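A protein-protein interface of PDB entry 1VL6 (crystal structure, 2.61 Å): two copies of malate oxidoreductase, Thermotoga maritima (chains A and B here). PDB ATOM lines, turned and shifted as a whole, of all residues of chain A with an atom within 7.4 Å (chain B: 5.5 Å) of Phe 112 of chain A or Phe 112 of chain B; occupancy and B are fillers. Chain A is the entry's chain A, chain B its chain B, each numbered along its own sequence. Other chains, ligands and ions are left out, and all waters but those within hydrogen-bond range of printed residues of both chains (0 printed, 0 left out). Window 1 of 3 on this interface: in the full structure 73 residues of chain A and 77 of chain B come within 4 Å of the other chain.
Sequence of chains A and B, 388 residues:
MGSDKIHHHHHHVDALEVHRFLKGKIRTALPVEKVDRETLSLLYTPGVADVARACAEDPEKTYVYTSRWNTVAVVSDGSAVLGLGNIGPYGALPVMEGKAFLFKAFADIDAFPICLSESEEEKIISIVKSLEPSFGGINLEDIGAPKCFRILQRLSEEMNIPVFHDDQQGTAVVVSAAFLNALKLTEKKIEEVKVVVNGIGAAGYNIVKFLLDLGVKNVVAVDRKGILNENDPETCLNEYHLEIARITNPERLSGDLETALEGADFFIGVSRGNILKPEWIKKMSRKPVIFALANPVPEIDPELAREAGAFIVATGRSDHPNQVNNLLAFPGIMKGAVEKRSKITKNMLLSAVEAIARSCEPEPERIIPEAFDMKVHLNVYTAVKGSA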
ATOM      1  N   ILE A  26      -0.228  -8.658  11.088  1.00  0.00           N
ATOM      2  CA  ILE A  26       0.913  -9.338  11.721  1.00  0.00           C
ATOM      3  C   ILE A  26       1.904  -9.910  10.691  1.00  0.00           C
ATOM      4  O   ILE A  26       1.565 -10.816   9.878  1.00  0.00           O
ATOM      5  CB  ILE A  26       0.386 -10.516  12.614  1.00  0.00           C
ATOM      6  CG1 ILE A  26      -0.690  -9.985  13.560  1.00  0.00           C
ATOM      7  CG2 ILE A  26       1.575 -11.295  13.415  1.00  0.00           C
ATOM      8  CD1 ILE A  26      -0.599 -10.538  14.918  1.00  0.00           C
ATOM      9  N   ARG A  27       3.128  -9.380  10.714  1.00  0.00           N
ATOM     10  CA  ARG A  27       4.232  -9.940   9.917  1.00  0.00           C
ATOM     11  C   ARG A  27       5.174 -10.631  10.916  1.00  0.00           C
ATOM     12  O   ARG A  27       5.195 -10.254  12.103  1.00  0.00           O
ATOM     13  CB  ARG A  27       5.021  -8.818   9.200  1.00  0.00           C
ATOM     14  CG  ARG A  27       4.174  -7.772   8.415  1.00  0.00           C
ATOM     15  CD  ARG A  27       4.071  -8.026   6.863  1.00  0.00           C
ATOM     16  NE  ARG A  27       2.827  -7.515   6.271  1.00  0.00           N
ATOM     17  CZ  ARG A  27       1.586  -7.960   6.580  1.00  0.00           C
ATOM     18  NH1 ARG A  27       1.403  -8.923   7.473  1.00  0.00           N
ATOM     19  NH2 ARG A  27       0.516  -7.426   6.004  1.00  0.00           N
ATOM     20  N   THR A  28       5.934 -11.638  10.475  1.00  0.00           N
ATOM     21  CA  THR A  28       7.214 -11.918  11.113  1.00  0.00           C
ATOM     22  C   THR A  28       8.300 -11.362  10.198  1.00  0.00           C
ATOM     23  O   THR A  28       8.018 -10.897   9.113  1.00  0.00           O
ATOM     24  CB  THR A  28       7.436 -13.444  11.519  1.00  0.00           C
ATOM     25  OG1 THR A  28       7.414 -14.321  10.385  1.00  0.00           O
ATOM     26  CG2 THR A  28       6.321 -13.956  12.420  1.00  0.00           C
ATOM     27  N   SER A  67      13.679 -14.327  22.055  1.00  0.00           N
ATOM     28  CA  SER A  67      12.863 -13.145  22.010  1.00  0.00           C
ATOM     29  C   SER A  67      11.935 -13.026  23.201  1.00  0.00           C
ATOM     30  O   SER A  67      11.163 -12.065  23.287  1.00  0.00           O
ATOM     31  CB  SER A  67      11.999 -13.195  20.761  1.00  0.00           C
ATOM     32  OG  SER A  67      12.792 -13.334  19.596  1.00  0.00           O
ATOM     33  N   ASN A  70      10.723  -9.882  25.100  1.00  0.00           N
ATOM     34  CA  ASN A  70       9.916  -8.883  24.443  1.00  0.00           C
ATOM     35  C   ASN A  70       8.716  -9.463  23.712  1.00  0.00           C
ATOM     36  O   ASN A  70       8.194  -8.804  22.823  1.00  0.00           O
ATOM     37  CB  ASN A  70      10.829  -8.105  23.497  1.00  0.00           C
ATOM     38  CG  ASN A  70      10.173  -6.880  22.919  1.00  0.00           C
ATOM     39  OD1 ASN A  70       9.665  -6.019  23.634  1.00  0.00           O
ATOM     40  ND2 ASN A  70      10.166  -6.807  21.597  1.00  0.00           N
ATOM     41  N   THR A  71       8.261 -10.666  24.061  1.00  0.00           N
ATOM     42  CA  THR A  71       7.044 -11.209  23.428  1.00  0.00           C
ATOM     43  C   THR A  71       5.898 -11.325  24.396  1.00  0.00           C
ATOM     44  O   THR A  71       6.073 -11.590  25.560  1.00  0.00           O
ATOM     45  CB  THR A  71       7.265 -12.573  22.739  1.00  0.00           C
ATOM     46  OG1 THR A  71       7.610 -13.577  23.695  1.00  0.00           O
ATOM     47  CG2 THR A  71       8.455 -12.519  21.805  1.00  0.00           C
ATOM     48  N   VAL A  72       4.709 -11.103  23.904  1.00  0.00           N
ATOM     49  CA  VAL A  72       3.527 -11.036  24.739  1.00  0.00           C
ATOM     50  C   VAL A  72       2.404 -11.807  24.003  1.00  0.00           C
ATOM     51  O   VAL A  72       2.242 -11.678  22.789  1.00  0.00           O
ATOM     52  CB  VAL A  72       3.197  -9.552  25.036  1.00  0.00           C
ATOM     53  CG1 VAL A  72       1.701  -9.325  25.413  1.00  0.00           C
ATOM     54  CG2 VAL A  72       4.146  -9.034  26.118  1.00  0.00           C
ATOM     55  N   ALA A  73       1.681 -12.662  24.735  1.00  0.00           N
ATOM     56  CA  ALA A  73       0.542 -13.345  24.160  1.00  0.00           C
ATOM     57  C   ALA A  73      -0.686 -12.498  24.398  1.00  0.00           C
ATOM     58  O   ALA A  73      -0.892 -12.031  25.494  1.00  0.00           O
ATOM     59  CB  ALA A  73       0.378 -14.686  24.797  1.00  0.00           C
ATOM     60  N   VAL A  74      -1.471 -12.258  23.359  1.00  0.00           N
ATOM     61  CA  VAL A  74      -2.737 -11.557  23.503  1.00  0.00           C
ATOM     62  C   VAL A  74      -3.788 -12.653  23.478  1.00  0.00           C
ATOM     63  O   VAL A  74      -4.070 -13.245  22.445  1.00  0.00           O
ATOM     64  CB  VAL A  74      -2.978 -10.546  22.374  1.00  0.00           C
ATOM     65  CG1 VAL A  74      -4.319  -9.835  22.557  1.00  0.00           C
ATOM     66  CG2 VAL A  74      -1.843  -9.541  22.313  1.00  0.00           C
ATOM     67  N   VAL A  75      -4.361 -12.922  24.644  1.00  0.00           N
ATOM     68  CA  VAL A  75      -5.165 -14.132  24.853  1.00  0.00           C
ATOM     69  C   VAL A  75      -6.653 -13.801  24.968  1.00  0.00           C
ATOM     70  O   VAL A  75      -7.047 -13.050  25.840  1.00  0.00           O
ATOM     71  CB  VAL A  75      -4.688 -14.865  26.119  1.00  0.00           C
ATOM     72  CG1 VAL A  75      -5.559 -16.083  26.430  1.00  0.00           C
ATOM     73  CG2 VAL A  75      -3.208 -15.269  25.958  1.00  0.00           C
ATOM     74  N   MET A  96      -7.610  -9.150  17.978  1.00  0.00           N
ATOM     75  CA  MET A  96      -6.347  -9.391  18.666  1.00  0.00           C
ATOM     76  C   MET A  96      -5.149  -9.046  17.747  1.00  0.00           C
ATOM     77  O   MET A  96      -4.094  -8.644  18.205  1.00  0.00           O
ATOM     78  CB  MET A  96      -6.284 -10.817  19.182  1.00  0.00           C
ATOM     79  CG  MET A  96      -7.434 -11.239  20.112  1.00  0.00           C
ATOM     80  SD  MET A  96      -7.904  -9.866  21.443  1.00  0.00           S
ATOM     81  CE  MET A  96      -9.780  -9.875  21.359  1.00  0.00           C
ATOM     82  N   GLU A  97      -5.312  -9.193  16.443  1.00  0.00           N
ATOM     83  CA  GLU A  97      -4.286  -8.743  15.538  1.00  0.00           C
ATOM     84  C   GLU A  97      -4.103  -7.211  15.654  1.00  0.00           C
ATOM     85  O   GLU A  97      -3.003  -6.704  15.660  1.00  0.00           O
ATOM     86  CB  GLU A  97      -4.659  -9.123  14.111  1.00  0.00           C
ATOM     87  CG  GLU A  97      -4.349 -10.539  13.694  1.00  0.00           C
ATOM     88  CD  GLU A  97      -4.186 -10.705  12.183  1.00  0.00           C
ATOM     89  OE1 GLU A  97      -4.468  -9.770  11.401  1.00  0.00           O
ATOM     90  OE2 GLU A  97      -3.766 -11.793  11.756  1.00  0.00           O
ATOM     91  N   ALA A 100      -2.246  -6.505  18.706  1.00  0.00           N
ATOM     92  CA  ALA A 100      -0.839  -6.843  18.552  1.00  0.00           C
ATOM     93  C   ALA A 100      -0.160  -5.706  17.815  1.00  0.00           C
ATOM     94  O   ALA A 100       0.909  -5.283  18.210  1.00  0.00           O
ATOM     95  CB  ALA A 100      -0.667  -8.142  17.807  1.00  0.00           C
ATOM     96  N   PHE A 103       0.588  -2.970  20.206  1.00  0.00           N
ATOM     97  CA  PHE A 103       1.669  -3.342  21.070  1.00  0.00           C
ATOM     98  C   PHE A 103       2.988  -3.041  20.399  1.00  0.00           C
ATOM     99  O   PHE A 103       3.880  -2.473  21.041  1.00  0.00           O
ATOM    100  CB  PHE A 103       1.600  -4.831  21.489  1.00  0.00           C
ATOM    101  CG  PHE A 103       0.902  -5.058  22.790  1.00  0.00           C
ATOM    102  CD1 PHE A 103       1.422  -4.532  23.965  1.00  0.00           C
ATOM    103  CD2 PHE A 103      -0.274  -5.771  22.845  1.00  0.00           C
ATOM    104  CE1 PHE A 103       0.765  -4.707  25.178  1.00  0.00           C
ATOM    105  CE2 PHE A 103      -0.943  -5.923  24.046  1.00  0.00           C
ATOM    106  CZ  PHE A 103      -0.424  -5.388  25.214  1.00  0.00           C
ATOM    107  N   ILE A 109       6.685  -3.932  21.294  1.00  0.00           N
ATOM    108  CA  ILE A 109       6.546  -5.284  21.849  1.00  0.00           C
ATOM    109  C   ILE A 109       6.077  -6.202  20.752  1.00  0.00           C
ATOM    110  O   ILE A 109       5.193  -5.840  19.973  1.00  0.00           O
ATOM    111  CB  ILE A 109       5.548  -5.285  22.998  1.00  0.00           C
ATOM    112  CG1 ILE A 109       6.208  -4.685  24.223  1.00  0.00           C
ATOM    113  CG2 ILE A 109       5.041  -6.675  23.296  1.00  0.00           C
ATOM    114  CD1 ILE A 109       5.257  -4.600  25.374  1.00  0.00           C
ATOM    115  N   ASP A 110       6.682  -7.383  20.690  1.00  0.00           N
ATOM    116  CA  ASP A 110       6.296  -8.377  19.730  1.00  0.00           C
ATOM    117  C   ASP A 110       5.129  -9.156  20.323  1.00  0.00           C
ATOM    118  O   ASP A 110       5.302 -10.055  21.136  1.00  0.00           O
ATOM    119  CB  ASP A 110       7.483  -9.285  19.446  1.00  0.00           C
ATOM    120  CG  ASP A 110       8.563  -8.610  18.643  1.00  0.00           C
ATOM    121  OD1 ASP A 110       8.308  -7.650  17.877  1.00  0.00           O
ATOM    122  OD2 ASP A 110       9.722  -9.002  18.695  1.00  0.00           O
ATOM    123  N   ALA A 111       3.924  -8.813  19.937  1.00  0.00           N
ATOM    124  CA  ALA A 111       2.763  -9.447  20.507  1.00  0.00           C
ATOM    125  C   ALA A 111       2.134 -10.430  19.509  1.00  0.00           C
ATOM    126  O   ALA A 111       2.097 -10.161  18.335  1.00  0.00           O
ATOM    127  CB  ALA A 111       1.774  -8.371  20.926  1.00  0.00           C
ATOM    128  N   PHE A 112       1.666 -11.576  20.008  1.00  0.00           N
ATOM    129  CA  PHE A 112       1.075 -12.649  19.183  1.00  0.00           C
ATOM    130  C   PHE A 112      -0.364 -12.904  19.676  1.00  0.00           C
ATOM    131  O   PHE A 112      -0.602 -12.963  20.874  1.00  0.00           O
ATOM    132  CB  PHE A 112       1.937 -13.942  19.240  1.00  0.00           C
ATOM    133  CG  PHE A 112       3.363 -13.727  18.789  1.00  0.00           C
ATOM    134  CD1 PHE A 112       4.308 -13.192  19.661  1.00  0.00           C
ATOM    135  CD2 PHE A 112       3.739 -13.993  17.474  1.00  0.00           C
ATOM    136  CE1 PHE A 112       5.610 -12.930  19.240  1.00  0.00           C
ATOM    137  CE2 PHE A 112       5.046 -13.747  17.041  1.00  0.00           C
ATOM    138  CZ  PHE A 112       5.983 -13.215  17.931  1.00  0.00           C
ATOM    139  N   PRO A 113      -1.330 -12.980  18.766  1.00  0.00           N
ATOM    140  CA  PRO A 113      -2.678 -13.322  19.150  1.00  0.00           C
ATOM    141  C   PRO A 113      -2.840 -14.784  19.415  1.00  0.00           C
ATOM    142  O   PRO A 113      -2.463 -15.595  18.574  1.00  0.00           O
ATOM    143  CB  PRO A 113      -3.517 -12.961  17.932  1.00  0.00           C
ATOM    144  CG  PRO A 113      -2.614 -12.282  17.016  1.00  0.00           C
ATOM    145  CD  PRO A 113      -1.239 -12.633  17.336  1.00  0.00           C
ATOM    146  N   ILE A 114      -3.408 -15.091  20.582  1.00  0.00           N
ATOM    147  CA  ILE A 114      -3.761 -16.407  20.956  1.00  0.00           C
ATOM    148  C   ILE A 114      -5.228 -16.461  21.328  1.00  0.00           C
ATOM    149  O   ILE A 114      -5.618 -16.150  22.455  1.00  0.00           O
ATOM    150  CB  ILE A 114      -2.854 -16.847  22.058  1.00  0.00           C
ATOM    151  CG1 ILE A 114      -1.504 -17.199  21.439  1.00  0.00           C
ATOM    152  CG2 ILE A 114      -3.401 -18.111  22.744  1.00  0.00           C
ATOM    153  CD1 ILE A 114      -0.419 -17.185  22.426  1.00  0.00           C
ATOM    154  N   CYS A 115      -6.021 -16.831  20.334  1.00  0.00           N
ATOM    155  CA  CYS A 115      -7.443 -16.872  20.403  1.00  0.00           C
ATOM    156  C   CYS A 115      -7.867 -18.331  20.531  1.00  0.00           C
ATOM    157  O   CYS A 115      -7.662 -19.163  19.610  1.00  0.00           O
ATOM    158  CB  CYS A 115      -8.016 -16.271  19.119  1.00  0.00           C
ATOM    159  SG  CYS A 115      -7.977 -14.449  19.009  1.00  0.00           S
ATOM    160  N   SER A 134       6.822 -19.735  26.578  1.00  0.00           N
ATOM    161  CA  SER A 134       6.872 -19.125  25.244  1.00  0.00           C
ATOM    162  C   SER A 134       6.741 -17.601  25.222  1.00  0.00           C
ATOM    163  O   SER A 134       6.924 -16.977  24.156  1.00  0.00           O
ATOM    164  CB  SER A 134       5.791 -19.779  24.365  1.00  0.00           C
ATOM    165  OG  SER A 134       5.996 -21.197  24.330  1.00  0.00           O
ATOM    166  N   PHE A 135       6.459 -16.999  26.384  1.00  0.00           N
ATOM    167  CA  PHE A 135       6.208 -15.552  26.454  1.00  0.00           C
ATOM    168  C   PHE A 135       6.838 -14.880  27.633  1.00  0.00           C
ATOM    169  O   PHE A 135       7.069 -15.489  28.660  1.00  0.00           O
ATOM    170  CB  PHE A 135       4.719 -15.286  26.485  1.00  0.00           C
ATOM    171  CG  PHE A 135       4.011 -15.805  25.284  1.00  0.00           C
ATOM    172  CD1 PHE A 135       4.076 -15.134  24.103  1.00  0.00           C
ATOM    173  CD2 PHE A 135       3.318 -17.008  25.334  1.00  0.00           C
ATOM    174  CE1 PHE A 135       3.434 -15.640  22.994  1.00  0.00           C
ATOM    175  CE2 PHE A 135       2.687 -17.510  24.241  1.00  0.00           C
ATOM    176  CZ  PHE A 135       2.766 -16.836  23.062  1.00  0.00           C
ATOM    177  N   ASN A 139      -1.272 -10.821  27.978  1.00  0.00           N
ATOM    178  CA  ASN A 139      -2.312  -9.829  27.950  1.00  0.00           C
ATOM    179  C   ASN A 139      -3.644 -10.502  27.709  1.00  0.00           C
ATOM    180  O   ASN A 139      -3.952 -10.913  26.591  1.00  0.00           O
ATOM    181  CB  ASN A 139      -2.041  -8.804  26.858  1.00  0.00           C
ATOM    182  CG  ASN A 139      -3.158  -7.759  26.737  1.00  0.00           C
ATOM    183  OD1 ASN A 139      -3.432  -7.311  25.637  1.00  0.00           O
ATOM    184  ND2 ASN A 139      -3.801  -7.390  27.851  1.00  0.00           N
ATOM    185  N   ILE B  26      13.335 -14.216  16.141  1.00  0.00           N
ATOM    186  CA  ILE B  26      11.957 -13.875  15.822  1.00  0.00           C
ATOM    187  C   ILE B  26      11.694 -12.363  15.984  1.00  0.00           C
ATOM    188  O   ILE B  26      11.886 -11.800  17.058  1.00  0.00           O
ATOM    189  CB  ILE B  26      11.015 -14.757  16.752  1.00  0.00           C
ATOM    190  CG1 ILE B  26      10.429 -15.891  15.909  1.00  0.00           C
ATOM    191  CG2 ILE B  26       9.868 -13.924  17.492  1.00  0.00           C
ATOM    192  CD1 ILE B  26      10.110 -17.095  16.674  1.00  0.00           C
ATOM    193  N   ARG B  27      11.284 -11.713  14.903  1.00  0.00           N
ATOM    194  CA  ARG B  27      10.789 -10.323  14.958  1.00  0.00           C
ATOM    195  C   ARG B  27       9.272 -10.366  14.645  1.00  0.00           C
ATOM    196  O   ARG B  27       8.800 -11.311  14.004  1.00  0.00           O
ATOM    197  CB  ARG B  27      11.527  -9.448  13.895  1.00  0.00           C
ATOM    198  CG  ARG B  27      13.090  -9.686  13.764  1.00  0.00           C
ATOM    199  CD  ARG B  27      13.944  -8.590  14.421  1.00  0.00           C
ATOM    200  NE  ARG B  27      15.302  -9.007  14.781  1.00  0.00           N
ATOM    201  CZ  ARG B  27      15.640  -9.770  15.848  1.00  0.00           C
ATOM    202  NH1 ARG B  27      14.719 -10.279  16.669  1.00  0.00           N
ATOM    203  NH2 ARG B  27      16.925 -10.043  16.075  1.00  0.00           N
ATOM    204  N   THR B  28       8.505  -9.367  15.076  1.00  0.00           N
ATOM    205  CA  THR B  28       7.297  -9.008  14.319  1.00  0.00           C
ATOM    206  C   THR B  28       7.592  -7.715  13.555  1.00  0.00           C
ATOM    207  O   THR B  28       8.661  -7.092  13.707  1.00  0.00           O
ATOM    208  CB  THR B  28       5.982  -8.943  15.173  1.00  0.00           C
ATOM    209  OG1 THR B  28       6.109  -8.002  16.256  1.00  0.00           O
ATOM    210  CG2 THR B  28       5.658 -10.328  15.851  1.00  0.00           C
ATOM    211  N   VAL B  72       1.752 -20.532  11.411  1.00  0.00           N
ATOM    212  CA  VAL B  72       1.937 -21.902  11.810  1.00  0.00           C
ATOM    213  C   VAL B  72       2.475 -21.918  13.217  1.00  0.00           C
ATOM    214  O   VAL B  72       3.377 -21.156  13.534  1.00  0.00           O
ATOM    215  CB  VAL B  72       2.913 -22.590  10.858  1.00  0.00           C
ATOM    216  CG1 VAL B  72       3.462 -23.923  11.423  1.00  0.00           C
ATOM    217  CG2 VAL B  72       2.252 -22.791   9.525  1.00  0.00           C
ATOM    218  N   ALA B  73       1.909 -22.770  14.071  1.00  0.00           N
ATOM    219  CA  ALA B  73       2.412 -22.891  15.436  1.00  0.00           C
ATOM    220  C   ALA B  73       3.457 -24.005  15.463  1.00  0.00           C
ATOM    221  O   ALA B  73       3.240 -25.070  14.889  1.00  0.00           O
ATOM    222  CB  ALA B  73       1.304 -23.173  16.384  1.00  0.00           C
ATOM    223  N   VAL B  74       4.605 -23.718  16.075  1.00  0.00           N
ATOM    224  CA  VAL B  74       5.663 -24.681  16.188  1.00  0.00           C
ATOM    225  C   VAL B  74       5.586 -25.218  17.598  1.00  0.00           C
ATOM    226  O   VAL B  74       6.041 -24.564  18.527  1.00  0.00           O
ATOM    227  CB  VAL B  74       7.000 -24.005  15.891  1.00  0.00           C
ATOM    228  CG1 VAL B  74       8.155 -24.920  16.220  1.00  0.00           C
ATOM    229  CG2 VAL B  74       7.065 -23.553  14.392  1.00  0.00           C
ATOM    230  N   ALA B 100      11.212 -21.658  13.445  1.00  0.00           N
ATOM    231  CA  ALA B 100      10.376 -20.561  12.917  1.00  0.00           C
ATOM    232  C   ALA B 100      11.150 -19.744  11.894  1.00  0.00           C
ATOM    233  O   ALA B 100      10.627 -19.395  10.843  1.00  0.00           O
ATOM    234  CB  ALA B 100       9.888 -19.661  14.006  1.00  0.00           C
ATOM    235  N   ASP B 110       4.818 -17.410   8.403  1.00  0.00           N
ATOM    236  CA  ASP B 110       4.977 -16.727   9.671  1.00  0.00           C
ATOM    237  C   ASP B 110       4.766 -17.744  10.756  1.00  0.00           C
ATOM    238  O   ASP B 110       3.632 -17.979  11.164  1.00  0.00           O
ATOM    239  CB  ASP B 110       3.948 -15.594   9.854  1.00  0.00           C
ATOM    240  CG  ASP B 110       4.095 -14.463   8.842  1.00  0.00           C
ATOM    241  OD1 ASP B 110       5.242 -14.030   8.551  1.00  0.00           O
ATOM    242  OD2 ASP B 110       3.093 -13.953   8.289  1.00  0.00           O
ATOM    243  N   ALA B 111       5.854 -18.342  11.243  1.00  0.00           N
ATOM    244  CA  ALA B 111       5.743 -19.392  12.256  1.00  0.00           C
ATOM    245  C   ALA B 111       6.064 -18.818  13.627  1.00  0.00           C
ATOM    246  O   ALA B 111       6.894 -17.918  13.758  1.00  0.00           O
ATOM    247  CB  ALA B 111       6.663 -20.529  11.922  1.00  0.00           C
ATOM    248  N   PHE B 112       5.455 -19.369  14.652  1.00  0.00           N
ATOM    249  CA  PHE B 112       5.652 -18.829  15.959  1.00  0.00           C
ATOM    250  C   PHE B 112       5.761 -19.972  16.964  1.00  0.00           C
ATOM    251  O   PHE B 112       4.945 -20.877  16.937  1.00  0.00           O
ATOM    252  CB  PHE B 112       4.526 -17.850  16.307  1.00  0.00           C
ATOM    253  CG  PHE B 112       4.692 -17.281  17.663  1.00  0.00           C
ATOM    254  CD1 PHE B 112       5.774 -16.434  17.932  1.00  0.00           C
ATOM    255  CD2 PHE B 112       3.868 -17.668  18.703  1.00  0.00           C
ATOM    256  CE1 PHE B 112       6.009 -15.934  19.218  1.00  0.00           C
ATOM    257  CE2 PHE B 112       4.093 -17.181  19.980  1.00  0.00           C
ATOM    258  CZ  PHE B 112       5.174 -16.304  20.237  1.00  0.00           C
ATOM    259  N   PRO B 113       6.759 -19.940  17.846  1.00  0.00           N
ATOM    260  CA  PRO B 113       7.002 -21.016  18.799  1.00  0.00           C
ATOM    261  C   PRO B 113       5.972 -21.109  19.896  1.00  0.00           C
ATOM    262  O   PRO B 113       5.701 -20.103  20.584  1.00  0.00           O
ATOM    263  CB  PRO B 113       8.325 -20.598  19.474  1.00  0.00           C
ATOM    264  CG  PRO B 113       8.892 -19.664  18.593  1.00  0.00           C
ATOM    265  CD  PRO B 113       7.737 -18.868  18.056  1.00  0.00           C
ATOM    266  N   ILE B 114       5.441 -22.311  20.081  1.00  0.00           N
ATOM    267  CA  ILE B 114       4.566 -22.604  21.214  1.00  0.00           C
ATOM    268  C   ILE B 114       5.154 -23.768  22.000  1.00  0.00           C
ATOM    269  O   ILE B 114       4.892 -24.944  21.715  1.00  0.00           O
ATOM    270  CB  ILE B 114       3.137 -22.939  20.736  1.00  0.00           C
ATOM    271  CG1 ILE B 114       2.500 -21.740  19.992  1.00  0.00           C
ATOM    272  CG2 ILE B 114       2.258 -23.411  21.913  1.00  0.00           C
ATOM    273  CD1 ILE B 114       2.260 -20.536  20.846  1.00  0.00           C
ATOM    274  N   PHE B 135      -4.326 -20.223  14.112  1.00  0.00           N
ATOM    275  CA  PHE B 135      -3.302 -20.653  13.143  1.00  0.00           C
ATOM    276  C   PHE B 135      -3.897 -21.333  11.950  1.00  0.00           C
ATOM    277  O   PHE B 135      -4.984 -21.864  12.006  1.00  0.00           O
ATOM    278  CB  PHE B 135      -2.316 -21.633  13.745  1.00  0.00           C
ATOM    279  CG  PHE B 135      -1.648 -21.132  14.934  1.00  0.00           C
ATOM    280  CD1 PHE B 135      -0.518 -20.358  14.824  1.00  0.00           C
ATOM    281  CD2 PHE B 135      -2.135 -21.433  16.187  1.00  0.00           C
ATOM    282  CE1 PHE B 135       0.120 -19.878  15.943  1.00  0.00           C
ATOM    283  CE2 PHE B 135      -1.479 -20.963  17.315  1.00  0.00           C
ATOM    284  CZ  PHE B 135      -0.343 -20.182  17.181  1.00  0.00           C
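OG1 of Thr 28 of chain A sits at hydrogen-bond distance from OD1 of Asp 110 of chain B (2.9 Å).
The side-chain hydroxyl (OG) of Ser 67 of chain A sits at hydrogen-bond distance from the backbone carbonyl oxygen (O) of Ile 26 of chain B, 3.1 Å away.
OG1 of Thr 28 of chain B lies within hydrogen-bond range of OD1 of Asp 110 of chain A, 2.8 Å away.
The backbone carbonyl oxygen (O) of Asn 70 of chain A lies within hydrogen-bond range of the backbone NH (N) of Asp 110 of chain A.
The side-chain hydroxyl (OG1) of Thr 71 of chain A lies within hydrogen-bond range of the backbone carbonyl oxygen (O) of Ser 134 of chain A, 3.5 Å away.
The backbone NH (N) of Val 72 of chain A lies within hydrogen-bond range of the backbone carbonyl oxygen (O) of Asp 110 of chain A (3.0 Å).
N of Val 74 of chain A sits at hydrogen-bond distance from O of Phe 112 of chain A.
N of Val 74 of chain B sits at hydrogen-bond distance from O of Phe 112 of chain B, 3.0 Å away.
O of Val 74 of chain B sits at hydrogen-bond distance from N of Ile 114 of chain B, 2.8 Å away.
Asp 110 of chain B touches Ile 26 of chain A (OD2 to O, 3.8 Å).
O of Arg 27 of chain A touches CA of Thr 28 of chain B, 3.3 Å away.
Arg 27 of chain B touches Thr 28 of chain A (O to CA, 3.4 Å).
Asp 110 of chain A touches Ile 26 of chain B.
CG2 of Ile 26 of chain B touches CZ of Phe 112 of chain A (3.97 Å).
CG2 of Thr 28 of chain B touches CZ of Phe 112 of chain A (3.6 Å).
Phe 112 of chain A touches Phe 112 of chain B.
Pro 113 of chain B touches Ser 134 of chain A (O to CB, 3.8 Å).
Ser 134 of chain A touches Ile 114 of chain B.
Phe 135 of chain A touches Phe 112 of chain B.
Of the printed residues of chain B, Arg 27 of chain A touches Thr 28.
Of the printed residues of chain B, Thr 28 of chain A touches Arg 27 (3.4 Å) and Asp 110 (2.9 Å).
Val 72 of chain A touches none of the printed residues of chain B.
Printed residues of chain B within 4 Å of Phe 112 of chain A: Ile 26, Thr 28 and Phe 112.
Of the printed residues of chain A, Phe 112 of chain B touches Phe 112 and Phe 135.
Printed residues of chain A within 4 Å of Pro 113 of chain B: Ser 134 (3.8 Å).
The nearest printed residue of chain A that does not touch Phe 112 of chain B is Ser 134 of chain A (4.3 Å).
Printed residues of chain B that touch a printed residue of chain A: Ile 26, Arg 27, Thr 28, Asp 110, Phe 112, Pro 113 and Ile 114.
Of the 24 printed residues of chain A, 8 touch a printed residue of chain B.
Hydrophobic or aromatic side chains of chain A that line the printed part of chain B: Phe 112 and Phe 135.
Along chain A the printed residues that touch a printed residue of chain B span positions 26 to 135.
Ile 26 of chain A touches Asp 110 of chain B, and with the chains exchanged Asp 110 of chain A touches Ile 26 of chain B.
Arg 27 of chain A touches Thr 28 of chain B, and with the chains exchanged Thr 28 of chain A touches Arg 27 of chain B.
Thr 28 of chain A touches Asp 110 of chain B, and with the chains exchanged Asp 110 of chain A touches Thr 28 of chain B.
Phe 135 of chain A touches Phe 112 of chain B, but with the chains exchanged Phe 112 of chain A does not touch Phe 135 of chain B (7.0 Å).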
